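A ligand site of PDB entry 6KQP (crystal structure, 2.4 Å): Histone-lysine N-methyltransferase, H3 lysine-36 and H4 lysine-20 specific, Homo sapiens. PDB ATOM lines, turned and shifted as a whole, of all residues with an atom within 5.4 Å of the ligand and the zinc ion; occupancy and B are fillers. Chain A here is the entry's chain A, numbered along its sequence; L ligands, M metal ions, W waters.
The side-chain hydroxyl (OH) of Tyr 134 sits at hydrogen-bond distance from an oxygen (O2) of the ligand.
An oxygen (O1) of the ligand lies within hydrogen-bond range of the backbone NH of Trp 91 (3.0 Å).
O of Arg 89 lies within hydrogen-bond range of N1 of the ligand (2.7 Å).
A nitrogen (N5) of the ligand sits at hydrogen-bond distance from the backbone NH (N) of Lys 208, 3.0 Å away.
OD1 of Asn 157 sits at hydrogen-bond distance from N1 of the ligand (2.9 Å).
The backbone carbonyl oxygen (O) of His 158 is in hydrogen-bond range of a nitrogen (N4) of the ligand (2.5 Å).
N4 of the ligand sits close to SG of Cys 207, at 3.4 Å.
The backbone carbonyl oxygen (O) of Thr 131 is in hydrogen-bond range of an oxygen (O5) of the ligand (2.7 Å).
The backbone carbonyl oxygen (O) of Trp 91 lies within hydrogen-bond range of a nitrogen (N1) of the ligand.
N of Phe 133 sits at hydrogen-bond distance from O4 of the ligand, at 3.1 Å.
The backbone NH of His 158 lies within hydrogen-bond range of a nitrogen (N3) of the ligand, at 2.8 Å.
O5 of the ligand sits at hydrogen-bond distance from OD1 of Asn 132, at 3.1 Å.
O4 of the ligand sits at hydrogen-bond distance from OD1 of Asn 202.
The backbone carbonyl oxygen (O) of Tyr 134 lies within hydrogen-bond range of the side-chain hydroxyl (OH) of Tyr 108.
A ring nitrogen (NE2) of His 158 lies within hydrogen-bond range of the backbone NH (N) of Cys 160 (3.5 Å).
The side-chain sulfur of Cys 214 lies close to the backbone NH of Gly 216, at 3.3 Å.
ND1 of His 158 lies within hydrogen-bond range of N of Tyr 195 (3.1 Å).
OH of Tyr 195 sits at hydrogen-bond distance from O of Met 156, 3.0 Å away.
The backbone carbonyl oxygen of Asn 202 lies within hydrogen-bond range of the side-chain hydroxyl of Thr 205 (2.9 Å).
O of Arg 89 lies close to OD1 of Asn 157 (3.3 Å).
The backbone NH of Ala 211 lies close to the side-chain sulfur of Cys 209, 3.5 Å away.
O of Arg 154 lies close to S1 of the ligand (3.6 Å).
Merely in contact with the ligand: Tyr 195 (3.4 Å), Val 206 (3.6 Å), Leu 218 (3.7 Å), Met 156 (3.7 Å), Phe 155 (3.7 Å) and Gly 90 (3.9 Å).
Hydrophobic or aromatic side chains that line the ligand: Trp 91, Tyr 134, Phe 155, His 158 and Leu 218.
The nearest printed residue that does not touch the ligand is Thr 205 (4.2 Å).
The nearest printed residue that does not touch the zinc ion is His 158 (4.1 Å).
The zinc ion is bound by SG of Cys 209 (2.2 Å), SG of Cys 214 (2.4 Å), SG of Cys 207 (2.4 Å) and SG of Cys 160 (2.5 Å).
The zinc ion has four donor atoms within binding distance.
Water W1 lies within hydrogen-bond range of the side-chain hydroxyl (OG1) of Thr 205 (2.5 Å), the backbone carbonyl oxygen (O) of Thr 131 (2.5 Å), the side-chain amide oxygen (OD1) of Asn 202 (2.7 Å) and an oxygen (O5) of the ligand (3.1 Å).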
ATOM      1  N   GLN A  88      17.366  -5.528 -27.150  1.00  0.00           N
ATOM      2  CA  GLN A  88      16.987  -4.836 -25.883  1.00  0.00           C
ATOM      3  C   GLN A  88      17.910  -5.204 -24.707  1.00  0.00           C
ATOM      4  O   GLN A  88      17.664  -4.718 -23.591  1.00  0.00           O
ATOM      5  CB  GLN A  88      15.545  -5.156 -25.475  1.00  0.00           C
ATOM      6  CG  GLN A  88      14.625  -5.573 -26.616  1.00  0.00           C
ATOM      7  CD  GLN A  88      13.241  -5.898 -26.110  1.00  0.00           C
ATOM      8  OE1 GLN A  88      12.673  -5.188 -25.296  1.00  0.00           O
ATOM      9  NE2 GLN A  88      12.682  -7.007 -26.592  1.00  0.00           N
ATOM     10  N   ARG A  89      18.940  -6.024 -24.926  1.00  0.00           N
ATOM     11  CA  ARG A  89      19.765  -6.584 -23.827  1.00  0.00           C
ATOM     12  C   ARG A  89      21.224  -6.155 -23.998  1.00  0.00           C
ATOM     13  O   ARG A  89      22.119  -6.848 -23.467  1.00  0.00           O
ATOM     14  CB  ARG A  89      19.619  -8.111 -23.811  1.00  0.00           C
ATOM     15  CG  ARG A  89      18.281  -8.582 -23.232  1.00  0.00           C
ATOM     16  CD  ARG A  89      17.986 -10.042 -23.540  1.00  0.00           C
ATOM     17  NE  ARG A  89      18.119 -10.306 -24.958  1.00  0.00           N
ATOM     18  CZ  ARG A  89      19.000 -11.124 -25.511  1.00  0.00           C
ATOM     19  NH1 ARG A  89      19.846 -11.832 -24.780  1.00  0.00           N
ATOM     20  NH2 ARG A  89      19.018 -11.234 -26.844  1.00  0.00           N
ATOM     21  N   GLY A  90      21.468  -5.038 -24.674  1.00  0.00           N
ATOM     22  CA  GLY A  90      22.820  -4.488 -24.888  1.00  0.00           C
ATOM     23  C   GLY A  90      23.642  -5.449 -25.709  1.00  0.00           C
ATOM     24  O   GLY A  90      23.097  -6.089 -26.637  1.00  0.00           O
ATOM     25  N   TRP A  91      24.921  -5.559 -25.361  1.00  0.00           N
ATOM     26  CA  TRP A  91      25.869  -6.468 -26.025  1.00  0.00           C
ATOM     27  C   TRP A  91      25.627  -7.910 -25.565  1.00  0.00           C
ATOM     28  O   TRP A  91      25.212  -8.141 -24.419  1.00  0.00           O
ATOM     29  CB  TRP A  91      27.296  -6.012 -25.779  1.00  0.00           C
ATOM     30  CG  TRP A  91      27.617  -4.704 -26.435  1.00  0.00           C
ATOM     31  CD1 TRP A  91      27.680  -3.477 -25.831  1.00  0.00           C
ATOM     32  CD2 TRP A  91      27.886  -4.494 -27.834  1.00  0.00           C
ATOM     33  NE1 TRP A  91      28.017  -2.532 -26.756  1.00  0.00           N
ATOM     34  CE2 TRP A  91      28.148  -3.125 -27.991  1.00  0.00           C
ATOM     35  CE3 TRP A  91      27.943  -5.329 -28.960  1.00  0.00           C
ATOM     36  CZ2 TRP A  91      28.465  -2.570 -29.233  1.00  0.00           C
ATOM     37  CZ3 TRP A  91      28.276  -4.783 -30.184  1.00  0.00           C
ATOM     38  CH2 TRP A  91      28.522  -3.416 -30.323  1.00  0.00           C
ATOM     39  N   GLY A  92      25.861  -8.853 -26.470  1.00  0.00           N
ATOM     40  CA  GLY A  92      25.572 -10.272 -26.237  1.00  0.00           C
ATOM     41  C   GLY A  92      26.737 -11.084 -26.713  1.00  0.00           C
ATOM     42  O   GLY A  92      27.598 -10.523 -27.393  1.00  0.00           O
ATOM     43  N   TYR A 108      33.848 -17.863 -16.433  1.00  0.00           N
ATOM     44  CA  TYR A 108      33.531 -16.468 -16.018  1.00  0.00           C
ATOM     45  C   TYR A 108      34.716 -15.919 -15.224  1.00  0.00           C
ATOM     46  O   TYR A 108      34.827 -16.205 -14.016  1.00  0.00           O
ATOM     47  CB  TYR A 108      32.225 -16.431 -15.228  1.00  0.00           C
ATOM     48  CG  TYR A 108      31.636 -15.044 -15.092  1.00  0.00           C
ATOM     49  CD1 TYR A 108      30.746 -14.563 -16.049  1.00  0.00           C
ATOM     50  CD2 TYR A 108      31.970 -14.213 -14.033  1.00  0.00           C
ATOM     51  CE1 TYR A 108      30.192 -13.302 -15.939  1.00  0.00           C
ATOM     52  CE2 TYR A 108      31.413 -12.956 -13.899  1.00  0.00           C
ATOM     53  CZ  TYR A 108      30.526 -12.499 -14.863  1.00  0.00           C
ATOM     54  OH  TYR A 108      29.988 -11.250 -14.790  1.00  0.00           O
ATOM     55  N   THR A 131      23.526   0.514 -15.537  1.00  0.00           N
ATOM     56  CA  THR A 131      22.600  -0.640 -15.391  1.00  0.00           C
ATOM     57  C   THR A 131      23.289  -1.951 -15.781  1.00  0.00           C
ATOM     58  O   THR A 131      22.605  -2.976 -15.719  1.00  0.00           O
ATOM     59  CB  THR A 131      21.346  -0.411 -16.246  1.00  0.00           C
ATOM     60  OG1 THR A 131      21.758  -0.265 -17.606  1.00  0.00           O
ATOM     61  CG2 THR A 131      20.588   0.817 -15.811  1.00  0.00           C
ATOM     62  N   ASN A 132      24.561  -1.916 -16.185  1.00  0.00           N
ATOM     63  CA  ASN A 132      25.327  -3.128 -16.550  1.00  0.00           C
ATOM     64  C   ASN A 132      26.177  -3.563 -15.353  1.00  0.00           C
ATOM     65  O   ASN A 132      27.100  -2.826 -14.967  1.00  0.00           O
ATOM     66  CB  ASN A 132      26.134  -2.921 -17.835  1.00  0.00           C
ATOM     67  CG  ASN A 132      25.287  -3.062 -19.081  1.00  0.00           C
ATOM     68  OD1 ASN A 132      24.263  -3.727 -19.084  1.00  0.00           O
ATOM     69  ND2 ASN A 132      25.737  -2.459 -20.178  1.00  0.00           N
ATOM     70  N   PHE A 133      25.855  -4.721 -14.768  1.00  0.00           N
ATOM     71  CA  PHE A 133      26.621  -5.344 -13.666  1.00  0.00           C
ATOM     72  C   PHE A 133      27.226  -6.678 -14.116  1.00  0.00           C
ATOM     73  O   PHE A 133      26.653  -7.392 -14.985  1.00  0.00           O
ATOM     74  CB  PHE A 133      25.706  -5.456 -12.440  1.00  0.00           C
ATOM     75  CG  PHE A 133      25.204  -4.125 -11.979  1.00  0.00           C
ATOM     76  CD1 PHE A 133      25.982  -3.327 -11.147  1.00  0.00           C
ATOM     77  CD2 PHE A 133      23.995  -3.624 -12.429  1.00  0.00           C
ATOM     78  CE1 PHE A 133      25.535  -2.073 -10.749  1.00  0.00           C
ATOM     79  CE2 PHE A 133      23.539  -2.367 -12.029  1.00  0.00           C
ATOM     80  CZ  PHE A 133      24.322  -1.600 -11.193  1.00  0.00           C
ATOM     81  N   TYR A 134      28.404  -6.978 -13.590  1.00  0.00           N
ATOM     82  CA  TYR A 134      29.242  -8.131 -14.007  1.00  0.00           C
ATOM     83  C   TYR A 134      29.736  -8.865 -12.768  1.00  0.00           C
ATOM     84  O   TYR A 134      30.855  -9.393 -12.771  1.00  0.00           O
ATOM     85  CB  TYR A 134      30.392  -7.654 -14.883  1.00  0.00           C
ATOM     86  CG  TYR A 134      29.978  -6.824 -16.063  1.00  0.00           C
ATOM     87  CD1 TYR A 134      29.722  -5.475 -15.919  1.00  0.00           C
ATOM     88  CD2 TYR A 134      29.839  -7.393 -17.331  1.00  0.00           C
ATOM     89  CE1 TYR A 134      29.332  -4.697 -17.001  1.00  0.00           C
ATOM     90  CE2 TYR A 134      29.452  -6.628 -18.423  1.00  0.00           C
ATOM     91  CZ  TYR A 134      29.195  -5.274 -18.257  1.00  0.00           C
ATOM     92  OH  TYR A 134      28.835  -4.496 -19.318  1.00  0.00           O
ATOM     93  N   ARG A 154      31.845 -12.383 -20.043  1.00  0.00           N
ATOM     94  CA  ARG A 154      31.220 -11.208 -19.368  1.00  0.00           C
ATOM     95  C   ARG A 154      30.033 -10.693 -20.205  1.00  0.00           C
ATOM     96  O   ARG A 154      29.241  -9.979 -19.638  1.00  0.00           O
ATOM     97  CB  ARG A 154      32.230 -10.081 -19.158  1.00  0.00           C
ATOM     98  CG  ARG A 154      32.521  -9.288 -20.422  1.00  0.00           C
ATOM     99  CD  ARG A 154      33.792  -8.468 -20.277  1.00  0.00           C
ATOM    100  NE  ARG A 154      33.645  -7.342 -19.377  1.00  0.00           N
ATOM    101  CZ  ARG A 154      33.006  -6.211 -19.669  1.00  0.00           C
ATOM    102  NH1 ARG A 154      32.421  -6.063 -20.848  1.00  0.00           N
ATOM    103  NH2 ARG A 154      32.949  -5.237 -18.779  1.00  0.00           N
ATOM    104  N   PHE A 155      29.951 -11.047 -21.493  1.00  0.00           N
ATOM    105  CA  PHE A 155      28.903 -10.593 -22.445  1.00  0.00           C
ATOM    106  C   PHE A 155      27.729 -11.568 -22.524  1.00  0.00           C
ATOM    107  O   PHE A 155      26.819 -11.340 -23.338  1.00  0.00           O
ATOM    108  CB  PHE A 155      29.508 -10.412 -23.838  1.00  0.00           C
ATOM    109  CG  PHE A 155      30.424  -9.219 -23.920  1.00  0.00           C
ATOM    110  CD1 PHE A 155      29.893  -7.939 -23.966  1.00  0.00           C
ATOM    111  CD2 PHE A 155      31.794  -9.362 -23.892  1.00  0.00           C
ATOM    112  CE1 PHE A 155      30.728  -6.835 -23.998  1.00  0.00           C
ATOM    113  CE2 PHE A 155      32.618  -8.263 -23.950  1.00  0.00           C
ATOM    114  CZ  PHE A 155      32.085  -6.992 -23.994  1.00  0.00           C
ATOM    115  N   MET A 156      27.733 -12.643 -21.741  1.00  0.00           N
ATOM    116  CA  MET A 156      26.618 -13.629 -21.745  1.00  0.00           C
ATOM    117  C   MET A 156      25.445 -13.077 -20.942  1.00  0.00           C
ATOM    118  O   MET A 156      25.644 -12.749 -19.764  1.00  0.00           O
ATOM    119  CB  MET A 156      27.052 -14.983 -21.181  1.00  0.00           C
ATOM    120  CG  MET A 156      27.920 -15.695 -22.189  1.00  0.00           C
ATOM    121  SD  MET A 156      28.509 -17.282 -21.670  1.00  0.00           S
ATOM    122  CE  MET A 156      26.965 -18.104 -21.290  1.00  0.00           C
ATOM    123  N   ASN A 157      24.287 -12.923 -21.580  1.00  0.00           N
ATOM    124  CA  ASN A 157      23.077 -12.321 -20.969  1.00  0.00           C
ATOM    125  C   ASN A 157      22.309 -13.364 -20.161  1.00  0.00           C
ATOM    126  O   ASN A 157      22.556 -14.581 -20.326  1.00  0.00           O
ATOM    127  CB  ASN A 157      22.139 -11.720 -22.016  1.00  0.00           C
ATOM    128  CG  ASN A 157      22.732 -10.471 -22.611  1.00  0.00           C
ATOM    129  OD1 ASN A 157      23.077  -9.555 -21.870  1.00  0.00           O
ATOM    130  ND2 ASN A 157      22.909 -10.454 -23.924  1.00  0.00           N
ATOM    131  N   HIS A 158      21.399 -12.899 -19.332  1.00  0.00           N
ATOM    132  CA  HIS A 158      20.450 -13.772 -18.622  1.00  0.00           C
ATOM    133  C   HIS A 158      19.322 -14.170 -19.568  1.00  0.00           C
ATOM    134  O   HIS A 158      18.836 -13.311 -20.348  1.00  0.00           O
ATOM    135  CB  HIS A 158      19.874 -13.094 -17.401  1.00  0.00           C
ATOM    136  CG  HIS A 158      18.688 -13.799 -16.876  1.00  0.00           C
ATOM    137  ND1 HIS A 158      18.786 -14.717 -15.865  1.00  0.00           N
ATOM    138  CD2 HIS A 158      17.387 -13.703 -17.212  1.00  0.00           C
ATOM    139  CE1 HIS A 158      17.567 -15.154 -15.574  1.00  0.00           C
ATOM    140  NE2 HIS A 158      16.680 -14.557 -16.400  1.00  0.00           N
ATOM    141  N   CYS A 159      18.894 -15.417 -19.440  1.00  0.00           N
ATOM    142  CA  CYS A 159      17.651 -15.951 -20.048  1.00  0.00           C
ATOM    143  C   CYS A 159      17.014 -16.911 -19.036  1.00  0.00           C
ATOM    144  O   CYS A 159      17.770 -17.709 -18.425  1.00  0.00           O
ATOM    145  CB  CYS A 159      17.947 -16.588 -21.399  1.00  0.00           C
ATOM    146  SG  CYS A 159      16.551 -17.452 -22.166  1.00  0.00           S
ATOM    147  N   CYS A 160      15.701 -16.809 -18.860  1.00  0.00           N
ATOM    148  CA  CYS A 160      14.897 -17.650 -17.932  1.00  0.00           C
ATOM    149  C   CYS A 160      14.716 -19.074 -18.482  1.00  0.00           C
ATOM    150  O   CYS A 160      14.384 -19.922 -17.665  1.00  0.00           O
ATOM    151  CB  CYS A 160      13.538 -17.028 -17.668  1.00  0.00           C
ATOM    152  SG  CYS A 160      13.590 -15.425 -16.821  1.00  0.00           S
ATOM    153  N   TYR A 195      20.826 -16.397 -14.324  1.00  0.00           N
ATOM    154  CA  TYR A 195      21.657 -15.760 -13.275  1.00  0.00           C
ATOM    155  C   TYR A 195      21.313 -16.367 -11.924  1.00  0.00           C
ATOM    156  O   TYR A 195      22.189 -16.386 -11.047  1.00  0.00           O
ATOM    157  CB  TYR A 195      21.450 -14.231 -13.295  1.00  0.00           C
ATOM    158  CG  TYR A 195      22.109 -13.531 -14.455  1.00  0.00           C
ATOM    159  CD1 TYR A 195      22.729 -14.240 -15.480  1.00  0.00           C
ATOM    160  CD2 TYR A 195      22.079 -12.152 -14.546  1.00  0.00           C
ATOM    161  CE1 TYR A 195      23.310 -13.590 -16.554  1.00  0.00           C
ATOM    162  CE2 TYR A 195      22.683 -11.479 -15.600  1.00  0.00           C
ATOM    163  CZ  TYR A 195      23.296 -12.204 -16.608  1.00  0.00           C
ATOM    164  OH  TYR A 195      23.902 -11.581 -17.654  1.00  0.00           O
ATOM    165  N   ASN A 202      21.495  -6.306 -10.007  1.00  0.00           N
ATOM    166  CA  ASN A 202      20.519  -6.187 -11.125  1.00  0.00           C
ATOM    167  C   ASN A 202      19.160  -5.689 -10.607  1.00  0.00           C
ATOM    168  O   ASN A 202      18.530  -4.934 -11.350  1.00  0.00           O
ATOM    169  CB  ASN A 202      20.467  -7.463 -11.956  1.00  0.00           C
ATOM    170  CG  ASN A 202      21.629  -7.492 -12.930  1.00  0.00           C
ATOM    171  OD1 ASN A 202      21.872  -6.509 -13.635  1.00  0.00           O
ATOM    172  ND2 ASN A 202      22.347  -8.612 -12.960  1.00  0.00           N
ATOM    173  N   THR A 205      15.852  -4.539 -12.711  1.00  0.00           N
ATOM    174  CA  THR A 205      15.959  -4.595 -14.190  1.00  0.00           C
ATOM    175  C   THR A 205      14.937  -5.602 -14.715  1.00  0.00           C
ATOM    176  O   THR A 205      14.847  -6.695 -14.142  1.00  0.00           O
ATOM    177  CB  THR A 205      17.340  -5.021 -14.698  1.00  0.00           C
ATOM    178  OG1 THR A 205      18.294  -4.147 -14.120  1.00  0.00           O
ATOM    179  CG2 THR A 205      17.413  -4.944 -16.210  1.00  0.00           C
ATOM    180  N   VAL A 206      14.190  -5.192 -15.742  1.00  0.00           N
ATOM    181  CA  VAL A 206      13.118  -6.011 -16.379  1.00  0.00           C
ATOM    182  C   VAL A 206      13.806  -6.941 -17.369  1.00  0.00           C
ATOM    183  O   VAL A 206      14.561  -6.464 -18.242  1.00  0.00           O
ATOM    184  CB  VAL A 206      12.054  -5.134 -17.072  1.00  0.00           C
ATOM    185  CG1 VAL A 206      11.098  -5.952 -17.924  1.00  0.00           C
ATOM    186  CG2 VAL A 206      11.272  -4.290 -16.069  1.00  0.00           C
ATOM    187  N   CYS A 207      13.526  -8.234 -17.252  1.00  0.00           N
ATOM    188  CA  CYS A 207      14.113  -9.253 -18.160  1.00  0.00           C
ATOM    189  C   CYS A 207      13.500  -9.071 -19.554  1.00  0.00           C
ATOM    190  O   CYS A 207      12.277  -8.971 -19.659  1.00  0.00           O
ATOM    191  CB  CYS A 207      13.913 -10.659 -17.615  1.00  0.00           C
ATOM    192  SG  CYS A 207      14.807 -11.879 -18.594  1.00  0.00           S
ATOM    193  N   LYS A 208      14.345  -9.064 -20.576  1.00  0.00           N
ATOM    194  CA  LYS A 208      13.928  -9.098 -22.002  1.00  0.00           C
ATOM    195  C   LYS A 208      14.442 -10.388 -22.664  1.00  0.00           C
ATOM    196  O   LYS A 208      14.791 -10.299 -23.832  1.00  0.00           O
ATOM    197  CB  LYS A 208      14.491  -7.881 -22.744  1.00  0.00           C
ATOM    198  CG  LYS A 208      14.119  -6.528 -22.155  1.00  0.00           C
ATOM    199  CD  LYS A 208      12.638  -6.260 -22.126  1.00  0.00           C
ATOM    200  CE  LYS A 208      12.304  -4.865 -21.638  1.00  0.00           C
ATOM    201  NZ  LYS A 208      10.849  -4.680 -21.428  1.00  0.00           N
ATOM    202  N   CYS A 209      14.520 -11.512 -21.947  1.00  0.00           N
ATOM    203  CA  CYS A 209      15.107 -12.773 -22.491  1.00  0.00           C
ATOM    204  C   CYS A 209      14.273 -13.298 -23.681  1.00  0.00           C
ATOM    205  O   CYS A 209      14.873 -13.904 -24.595  1.00  0.00           O
ATOM    206  CB  CYS A 209      15.297 -13.847 -21.423  1.00  0.00           C
ATOM    207  SG  CYS A 209      13.784 -14.560 -20.713  1.00  0.00           S
ATOM    208  N   GLY A 210      12.958 -13.097 -23.689  1.00  0.00           N
ATOM    209  CA  GLY A 210      12.073 -13.546 -24.773  1.00  0.00           C
ATOM    210  C   GLY A 210      11.655 -14.992 -24.601  1.00  0.00           C
ATOM    211  O   GLY A 210      11.098 -15.544 -25.562  1.00  0.00           O
ATOM    212  N   ALA A 211      11.915 -15.592 -23.431  1.00  0.00           N
ATOM    213  CA  ALA A 211      11.549 -16.991 -23.125  1.00  0.00           C
ATOM    214  C   ALA A 211      10.093 -17.068 -22.712  1.00  0.00           C
ATOM    215  O   ALA A 211       9.617 -16.206 -21.987  1.00  0.00           O
ATOM    216  CB  ALA A 211      12.438 -17.557 -22.052  1.00  0.00           C
ATOM    217  N   CYS A 214       9.371 -16.635 -18.958  1.00  0.00           N
ATOM    218  CA  CYS A 214      10.138 -15.481 -18.419  1.00  0.00           C
ATOM    219  C   CYS A 214       9.460 -14.904 -17.169  1.00  0.00           C
ATOM    220  O   CYS A 214       8.287 -14.530 -17.236  1.00  0.00           O
ATOM    221  CB  CYS A 214      10.334 -14.388 -19.466  1.00  0.00           C
ATOM    222  SG  CYS A 214      11.197 -12.939 -18.813  1.00  0.00           S
ATOM    223  N   SER A 215      10.217 -14.765 -16.072  1.00  0.00           N
ATOM    224  CA  SER A 215       9.720 -14.254 -14.765  1.00  0.00           C
ATOM    225  C   SER A 215       9.672 -12.717 -14.778  1.00  0.00           C
ATOM    226  O   SER A 215       9.128 -12.130 -13.818  1.00  0.00           O
ATOM    227  CB  SER A 215      10.610 -14.763 -13.671  1.00  0.00           C
ATOM    228  OG  SER A 215      11.770 -13.959 -13.575  1.00  0.00           O
ATOM    229  N   GLY A 216      10.259 -12.075 -15.798  1.00  0.00           N
ATOM    230  CA  GLY A 216      10.437 -10.616 -15.859  1.00  0.00           C
ATOM    231  C   GLY A 216      11.588 -10.095 -14.990  1.00  0.00           C
ATOM    232  O   GLY A 216      11.814  -8.880 -14.993  1.00  0.00           O
ATOM    233  N   PHE A 217      12.326 -10.962 -14.293  1.00  0.00           N
ATOM    234  CA  PHE A 217      13.520 -10.593 -13.502  1.00  0.00           C
ATOM    235  C   PHE A 217      14.749 -11.363 -13.980  1.00  0.00           C
ATOM    236  O   PHE A 217      14.630 -12.412 -14.616  1.00  0.00           O
ATOM    237  CB  PHE A 217      13.292 -10.859 -12.011  1.00  0.00           C
ATOM    238  CG  PHE A 217      12.225  -9.997 -11.398  1.00  0.00           C
ATOM    239  CD1 PHE A 217      12.502  -8.679 -11.045  1.00  0.00           C
ATOM    240  CD2 PHE A 217      10.946 -10.492 -11.170  1.00  0.00           C
ATOM    241  CE1 PHE A 217      11.517  -7.869 -10.468  1.00  0.00           C
ATOM    242  CE2 PHE A 217       9.977  -9.692 -10.576  1.00  0.00           C
ATOM    243  CZ  PHE A 217      10.262  -8.385 -10.224  1.00  0.00           C
ATOM    244  N   LEU A 218      15.929 -10.816 -13.691  1.00  0.00           N
ATOM    245  CA  LEU A 218      17.228 -11.510 -13.948  1.00  0.00           C
ATOM    246  C   LEU A 218      17.523 -12.395 -12.729  1.00  0.00           C
ATOM    247  O   LEU A 218      18.280 -11.953 -11.832  1.00  0.00           O
ATOM    248  CB  LEU A 218      18.332 -10.478 -14.180  1.00  0.00           C
ATOM    249  CG  LEU A 218      18.509  -9.971 -15.617  1.00  0.00           C
ATOM    250  CD1 LEU A 218      17.197  -9.546 -16.230  1.00  0.00           C
ATOM    251  CD2 LEU A 218      19.517  -8.832 -15.652  1.00  0.00           C
HETATM  252  N1  LIG L   1      24.422  -6.986 -22.105  1.00  0.00           N
HETATM  253  C1  LIG L   1      25.638  -6.826 -21.262  1.00  0.00           C
HETATM  254  C2  LIG L   1      26.542  -5.761 -21.900  1.00  0.00           C
HETATM  255  O1  LIG L   1      25.986  -4.910 -22.627  1.00  0.00           O
HETATM  256  O2  LIG L   1      27.763  -5.792 -21.642  1.00  0.00           O
HETATM  257  C3  LIG L   1      26.364  -8.176 -21.121  1.00  0.00           C
HETATM  258  C4  LIG L   1      25.789  -9.022 -19.991  1.00  0.00           C
HETATM  259  S1  LIG L   1      26.243  -8.339 -18.371  1.00  0.00           S
HETATM  260  C5  LIG L   1      26.964  -9.782 -17.571  1.00  0.00           C
HETATM  261  C6  LIG L   1      24.667  -8.320 -17.528  1.00  0.00           C
HETATM  262  C7  LIG L   1      23.879  -7.055 -17.749  1.00  0.00           C
HETATM  263  O3  LIG L   1      23.261  -7.093 -19.067  1.00  0.00           O
HETATM  264  C8  LIG L   1      22.759  -6.885 -16.731  1.00  0.00           C
HETATM  265  O4  LIG L   1      23.222  -6.091 -15.654  1.00  0.00           O
HETATM  266  C9  LIG L   1      21.653  -6.225 -17.564  1.00  0.00           C
HETATM  267  O5  LIG L   1      21.768  -4.824 -17.521  1.00  0.00           O
HETATM  268  C10 LIG L   1      21.892  -6.784 -18.972  1.00  0.00           C
HETATM  269  N2  LIG L   1      21.121  -7.990 -19.225  1.00  0.00           N
HETATM  270  C11 LIG L   1      21.600  -9.283 -19.220  1.00  0.00           C
HETATM  271  N3  LIG L   1      20.675 -10.187 -19.442  1.00  0.00           N
HETATM  272  C12 LIG L   1      19.512  -9.447 -19.581  1.00  0.00           C
HETATM  273  C13 LIG L   1      18.166  -9.828 -19.809  1.00  0.00           C
HETATM  274  N4  LIG L   1      17.767 -11.083 -19.946  1.00  0.00           N
HETATM  275  N5  LIG L   1      17.239  -8.843 -19.863  1.00  0.00           N
HETATM  276  C14 LIG L   1      17.651  -7.570 -19.735  1.00  0.00           C
HETATM  277  N6  LIG L   1      18.874  -7.090 -19.518  1.00  0.00           N
HETATM  278  C15 LIG L   1      19.773  -8.095 -19.437  1.00  0.00           C
HETATM  279 ZN    ZN M   1      13.404 -13.813 -18.729  1.00  0.00          ZN
HETATM  280  O   HOH W   1      20.707  -4.261 -14.661  1.00  0.00           O
